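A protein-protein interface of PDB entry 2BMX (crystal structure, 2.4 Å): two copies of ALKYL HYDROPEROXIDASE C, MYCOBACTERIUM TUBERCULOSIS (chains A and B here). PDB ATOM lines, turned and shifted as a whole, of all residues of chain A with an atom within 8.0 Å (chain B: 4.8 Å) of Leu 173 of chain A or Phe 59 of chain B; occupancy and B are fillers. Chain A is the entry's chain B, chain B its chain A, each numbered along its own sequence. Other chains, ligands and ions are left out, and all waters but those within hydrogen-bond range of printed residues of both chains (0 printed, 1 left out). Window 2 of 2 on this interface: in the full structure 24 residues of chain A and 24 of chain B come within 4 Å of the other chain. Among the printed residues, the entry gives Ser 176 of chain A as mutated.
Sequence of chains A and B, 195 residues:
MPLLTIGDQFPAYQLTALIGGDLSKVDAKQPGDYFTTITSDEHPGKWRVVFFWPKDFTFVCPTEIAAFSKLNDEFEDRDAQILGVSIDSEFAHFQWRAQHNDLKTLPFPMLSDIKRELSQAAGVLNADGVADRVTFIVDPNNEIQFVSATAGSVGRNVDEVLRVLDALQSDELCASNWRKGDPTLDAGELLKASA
O of Gly 155 of chain B is in hydrogen-bond range of NH2 of Arg 163 of chain A. The backbone carbonyl oxygen (O) of Glu 172 of chain A lies close to the backbone carbonyl oxygen (O) of Ser 153 of chain B (3.4 Å). The backbone carbonyl oxygen (O) of Leu 173 of chain A sits close to the backbone NH (N) of Gly 155 of chain B, 3.4 Å away. SG of Cys 61 of chain B forms a disulfide with SG of Cys 174 of chain A (2.1 Å). The side-chain sulfur (SG) of Cys 61 of chain B sits close to the backbone carbonyl oxygen (O) of Leu 173 of chain A (3.2 Å).
N of Glu 172 of chain A is in hydrogen-bond range of OG of Ser 170 of chain A (3.2 Å). ND2 of Asn 177 of chain A lies within hydrogen-bond range of OE1 of Glu 172 of chain A (3.0 Å). The backbone NH of Cys 174 of chain A is in hydrogen-bond range of the side-chain carboxylate of Glu 172 of chain A.
Among the printed residues, pairs that only touch across the chains: Arg 163 of chain A with Val 154 of chain B, Ala 167 of chain A with Val 154 of chain B, Leu 173 of chain A with Phe 59 of chain B, Leu 173 of chain A with Ser 153 of chain B and Cys 174 of chain A with Phe 59 of chain B.
Of chain B, only Phe 59 (3.5 Å), Cys 61 (3.2 Å), Ser 153 (3.6 Å) and Gly 155 (3.3 Å) come within 4 Å of Leu 173 of chain A. Ser 176 of chain A touches none of the printed residues of chain B. Thr 58 of chain B touches none of the printed residues of chain A. Of the printed residues of chain A, Phe 59 of chain B touches Leu 173 and Cys 174. Of the printed residues of chain A, Cys 61 of chain B touches Leu 173 (3.2 Å) and Cys 174 (2.1 Å). Of the printed residues of chain A, Gly 155 of chain B touches Arg 163 (2.5 Å) and Leu 173 (3.3 Å). The nearest residue of chain B that does not touch Leu 173 of chain A is Val 154 of chain B (4.5 Å). The nearest printed residue of chain A that does not touch Phe 59 of chain B is Glu 172 of chain A (6.8 Å). The nearest printed residue of chain A that does not touch Ser 153 of chain B is Ala 167 of chain A (5.4 Å).
Hydrophobic or aromatic side chains of chain B within 4 Å of the printed part of chain A: Phe 59 and Val 154. Of the 10 printed residues of chain A, 5 touch a printed residue of chain B. Printed residues of chain A that touch a printed residue of chain B: Arg 163, Ala 167, Glu 172, Leu 173 and Cys 174. Along chain A the printed residues that touch a printed residue of chain B span positions 163 to 174. Among the printed residues, no Asp or Glu carboxylate lies within 4 Å of a Lys or Arg side-chain nitrogen of the other chain.
No position is printed for both chains.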
ATOM      1  N   ARG A 163      11.727 -11.880  12.652  1.00  0.00           N
ATOM      2  CA  ARG A 163      11.119 -11.526  13.936  1.00  0.00           C
ATOM      3  C   ARG A 163      10.008 -12.508  14.377  1.00  0.00           C
ATOM      4  O   ARG A 163       9.977 -13.029  15.500  1.00  0.00           O
ATOM      5  CB  ARG A 163      10.517 -10.145  13.777  1.00  0.00           C
ATOM      6  CG  ARG A 163      10.131  -9.476  15.066  1.00  0.00           C
ATOM      7  CD  ARG A 163       9.000  -8.481  14.792  1.00  0.00           C
ATOM      8  NE  ARG A 163       8.027  -8.801  15.805  1.00  0.00           N
ATOM      9  CZ  ARG A 163       6.736  -9.037  15.659  1.00  0.00           C
ATOM     10  NH1 ARG A 163       6.070  -8.899  14.512  1.00  0.00           N
ATOM     11  NH2 ARG A 163       6.114  -9.363  16.773  1.00  0.00           N
ATOM     12  N   ALA A 167       9.982 -14.886  17.447  1.00  0.00           N
ATOM     13  CA  ALA A 167       8.923 -14.818  18.454  1.00  0.00           C
ATOM     14  C   ALA A 167       8.209 -16.192  18.587  1.00  0.00           C
ATOM     15  O   ALA A 167       7.870 -16.602  19.704  1.00  0.00           O
ATOM     16  CB  ALA A 167       7.951 -13.683  18.163  1.00  0.00           C
ATOM     17  N   SER A 170      10.439 -18.434  20.806  1.00  0.00           N
ATOM     18  CA  SER A 170      10.945 -17.895  22.053  1.00  0.00           C
ATOM     19  C   SER A 170       9.873 -17.348  22.979  1.00  0.00           C
ATOM     20  O   SER A 170      10.193 -16.959  24.114  1.00  0.00           O
ATOM     21  CB  SER A 170      11.975 -16.781  21.768  1.00  0.00           C
ATOM     22  OG  SER A 170      11.380 -15.495  21.642  1.00  0.00           O
ATOM     23  N   ASP A 171       8.622 -17.280  22.501  1.00  0.00           N
ATOM     24  CA  ASP A 171       7.553 -16.567  23.250  1.00  0.00           C
ATOM     25  C   ASP A 171       7.968 -15.122  23.734  1.00  0.00           C
ATOM     26  O   ASP A 171       7.719 -14.733  24.889  1.00  0.00           O
ATOM     27  CB  ASP A 171       7.022 -17.391  24.470  1.00  0.00           C
ATOM     28  CG  ASP A 171       6.869 -18.912  24.184  1.00  0.00           C
ATOM     29  OD1 ASP A 171       6.385 -19.310  23.078  1.00  0.00           O
ATOM     30  OD2 ASP A 171       7.237 -19.706  25.097  1.00  0.00           O
ATOM     31  N   GLU A 172       8.645 -14.368  22.857  1.00  0.00           N
ATOM     32  CA  GLU A 172       8.691 -12.920  22.959  1.00  0.00           C
ATOM     33  C   GLU A 172       7.293 -12.473  22.570  1.00  0.00           C
ATOM     34  O   GLU A 172       6.776 -12.906  21.546  1.00  0.00           O
ATOM     35  CB  GLU A 172       9.719 -12.315  21.990  1.00  0.00           C
ATOM     36  CG  GLU A 172       9.694 -10.764  21.915  1.00  0.00           C
ATOM     37  CD  GLU A 172       9.948 -10.075  23.254  1.00  0.00           C
ATOM     38  OE1 GLU A 172       9.093  -9.284  23.724  1.00  0.00           O
ATOM     39  OE2 GLU A 172      11.014 -10.326  23.856  1.00  0.00           O
ATOM     40  N   LEU A 173       6.694 -11.622  23.396  1.00  0.00           N
ATOM     41  CA  LEU A 173       5.367 -11.065  23.148  1.00  0.00           C
ATOM     42  C   LEU A 173       5.368  -9.710  22.416  1.00  0.00           C
ATOM     43  O   LEU A 173       4.325  -9.284  21.931  1.00  0.00           O
ATOM     44  CB  LEU A 173       4.607 -10.904  24.486  1.00  0.00           C
ATOM     45  CG  LEU A 173       4.561 -12.097  25.449  1.00  0.00           C
ATOM     46  CD1 LEU A 173       4.002 -11.674  26.783  1.00  0.00           C
ATOM     47  CD2 LEU A 173       3.800 -13.293  24.899  1.00  0.00           C
ATOM     48  N   CYS A 174       6.513  -9.031  22.354  1.00  0.00           N
ATOM     49  CA  CYS A 174       6.584  -7.622  21.891  1.00  0.00           C
ATOM     50  C   CYS A 174       7.343  -7.397  20.571  1.00  0.00           C
ATOM     51  O   CYS A 174       8.545  -7.670  20.474  1.00  0.00           O
ATOM     52  CB  CYS A 174       7.190  -6.738  22.981  1.00  0.00           C
ATOM     53  SG  CYS A 174       6.098  -6.503  24.377  1.00  0.00           S
ATOM     54  N   ALA A 175       6.653  -6.866  19.563  1.00  0.00           N
ATOM     55  CA  ALA A 175       7.342  -6.497  18.319  1.00  0.00           C
ATOM     56  C   ALA A 175       8.497  -5.482  18.549  1.00  0.00           C
ATOM     57  O   ALA A 175       9.501  -5.516  17.833  1.00  0.00           O
ATOM     58  CB  ALA A 175       6.346  -5.986  17.278  1.00  0.00           C
ATOM     59  N   SER A 176       8.354  -4.595  19.543  1.00  0.00           N
ATOM     60  CA  SER A 176       9.369  -3.579  19.855  1.00  0.00           C
ATOM     61  C   SER A 176      10.595  -4.104  20.611  1.00  0.00           C
ATOM     62  O   SER A 176      11.563  -3.376  20.793  1.00  0.00           O
ATOM     63  CB  SER A 176       8.758  -2.388  20.609  1.00  0.00           C
ATOM     64  OG  SER A 176       8.340  -2.752  21.917  1.00  0.00           O
ATOM     65  N   ASN A 177      10.558  -5.353  21.068  1.00  0.00           N
ATOM     66  CA  ASN A 177      11.725  -5.920  21.748  1.00  0.00           C
ATOM     67  C   ASN A 177      12.725  -6.529  20.753  1.00  0.00           C
ATOM     68  O   ASN A 177      13.869  -6.832  21.106  1.00  0.00           O
ATOM     69  CB  ASN A 177      11.315  -6.908  22.842  1.00  0.00           C
ATOM     70  CG  ASN A 177      11.004  -6.212  24.178  1.00  0.00           C
ATOM     71  OD1 ASN A 177      11.291  -5.024  24.377  1.00  0.00           O
ATOM     72  ND2 ASN A 177      10.411  -6.961  25.095  1.00  0.00           N
ATOM     73  N   PHE B  57      -8.440  -9.282  27.350  1.00  0.00           N
ATOM     74  CA  PHE B  57      -7.743  -9.527  28.646  1.00  0.00           C
ATOM     75  C   PHE B  57      -6.480 -10.406  28.604  1.00  0.00           C
ATOM     76  O   PHE B  57      -6.132 -10.999  29.579  1.00  0.00           O
ATOM     77  CB  PHE B  57      -8.701 -10.016  29.754  1.00  0.00           C
ATOM     78  CG  PHE B  57     -10.008  -9.275  29.785  1.00  0.00           C
ATOM     79  CD1 PHE B  57     -11.162  -9.842  29.218  1.00  0.00           C
ATOM     80  CD2 PHE B  57     -10.080  -7.990  30.313  1.00  0.00           C
ATOM     81  CE1 PHE B  57     -12.393  -9.135  29.182  1.00  0.00           C
ATOM     82  CE2 PHE B  57     -11.304  -7.294  30.321  1.00  0.00           C
ATOM     83  CZ  PHE B  57     -12.473  -7.885  29.750  1.00  0.00           C
ATOM     84  N   THR B  58      -5.828 -10.492  27.461  1.00  0.00           N
ATOM     85  CA  THR B  58      -4.564 -11.192  27.321  1.00  0.00           C
ATOM     86  C   THR B  58      -3.494 -10.087  27.153  1.00  0.00           C
ATOM     87  O   THR B  58      -3.836  -8.969  26.729  1.00  0.00           O
ATOM     88  CB  THR B  58      -4.614 -12.112  26.098  1.00  0.00           C
ATOM     89  OG1 THR B  58      -5.259 -11.407  25.050  1.00  0.00           O
ATOM     90  CG2 THR B  58      -5.497 -13.288  26.394  1.00  0.00           C
ATOM     91  N   PHE B  59      -2.236 -10.383  27.487  1.00  0.00           N
ATOM     92  CA  PHE B  59      -1.163  -9.384  27.392  1.00  0.00           C
ATOM     93  C   PHE B  59      -1.046  -8.730  26.021  1.00  0.00           C
ATOM     94  O   PHE B  59      -0.934  -9.409  24.993  1.00  0.00           O
ATOM     95  CB  PHE B  59       0.185  -9.969  27.787  1.00  0.00           C
ATOM     96  CG  PHE B  59       1.300  -8.955  27.832  1.00  0.00           C
ATOM     97  CD1 PHE B  59       1.522  -8.196  28.970  1.00  0.00           C
ATOM     98  CD2 PHE B  59       2.132  -8.758  26.731  1.00  0.00           C
ATOM     99  CE1 PHE B  59       2.559  -7.255  29.022  1.00  0.00           C
ATOM    100  CE2 PHE B  59       3.188  -7.825  26.775  1.00  0.00           C
ATOM    101  CZ  PHE B  59       3.391  -7.069  27.924  1.00  0.00           C
ATOM    102  N   VAL B  60      -1.103  -7.400  26.020  1.00  0.00           N
ATOM    103  CA  VAL B  60      -0.693  -6.618  24.851  1.00  0.00           C
ATOM    104  C   VAL B  60       0.453  -5.697  25.252  1.00  0.00           C
ATOM    105  O   VAL B  60       0.506  -5.221  26.387  1.00  0.00           O
ATOM    106  CB  VAL B  60      -1.838  -5.802  24.207  1.00  0.00           C
ATOM    107  CG1 VAL B  60      -1.333  -5.169  22.883  1.00  0.00           C
ATOM    108  CG2 VAL B  60      -3.057  -6.688  23.929  1.00  0.00           C
ATOM    109  N   CYS B  61       1.374  -5.463  24.322  1.00  0.00           N
ATOM    110  CA  CYS B  61       2.519  -4.601  24.604  1.00  0.00           C
ATOM    111  C   CYS B  61       2.118  -3.138  24.671  1.00  0.00           C
ATOM    112  O   CYS B  61       1.463  -2.652  23.744  1.00  0.00           O
ATOM    113  CB  CYS B  61       3.618  -4.778  23.550  1.00  0.00           C
ATOM    114  SG  CYS B  61       4.212  -6.488  23.457  1.00  0.00           S
ATOM    115  N   PRO B  62       2.513  -2.441  25.764  1.00  0.00           N
ATOM    116  CA  PRO B  62       2.364  -0.996  25.839  1.00  0.00           C
ATOM    117  C   PRO B  62       2.803  -0.291  24.545  1.00  0.00           C
ATOM    118  O   PRO B  62       2.102   0.619  24.086  1.00  0.00           O
ATOM    119  CB  PRO B  62       3.254  -0.626  27.028  1.00  0.00           C
ATOM    120  CG  PRO B  62       3.097  -1.795  27.939  1.00  0.00           C
ATOM    121  CD  PRO B  62       3.098  -2.981  27.008  1.00  0.00           C
ATOM    122  N   SER B 153       1.444 -16.089  20.453  1.00  0.00           N
ATOM    123  CA  SER B 153       1.422 -14.747  21.021  1.00  0.00           C
ATOM    124  C   SER B 153       2.568 -13.943  20.457  1.00  0.00           C
ATOM    125  O   SER B 153       3.420 -13.435  21.178  1.00  0.00           O
ATOM    126  CB  SER B 153       1.494 -14.812  22.563  1.00  0.00           C
ATOM    127  OG  SER B 153       0.178 -14.865  23.101  1.00  0.00           O
ATOM    128  N   VAL B 154       2.596 -13.894  19.142  1.00  0.00           N
ATOM    129  CA  VAL B 154       3.524 -13.103  18.406  1.00  0.00           C
ATOM    130  C   VAL B 154       2.894 -11.710  18.368  1.00  0.00           C
ATOM    131  O   VAL B 154       1.783 -11.551  17.877  1.00  0.00           O
ATOM    132  CB  VAL B 154       3.734 -13.709  16.975  1.00  0.00           C
ATOM    133  CG1 VAL B 154       4.524 -12.776  16.087  1.00  0.00           C
ATOM    134  CG2 VAL B 154       4.387 -15.076  17.104  1.00  0.00           C
ATOM    135  N   GLY B 155       3.608 -10.722  18.925  1.00  0.00           N
ATOM    136  CA  GLY B 155       3.195  -9.330  18.874  1.00  0.00           C
ATOM    137  C   GLY B 155       2.977  -8.780  17.476  1.00  0.00           C
ATOM    138  O   GLY B 155       3.670  -9.134  16.521  1.00  0.00           O
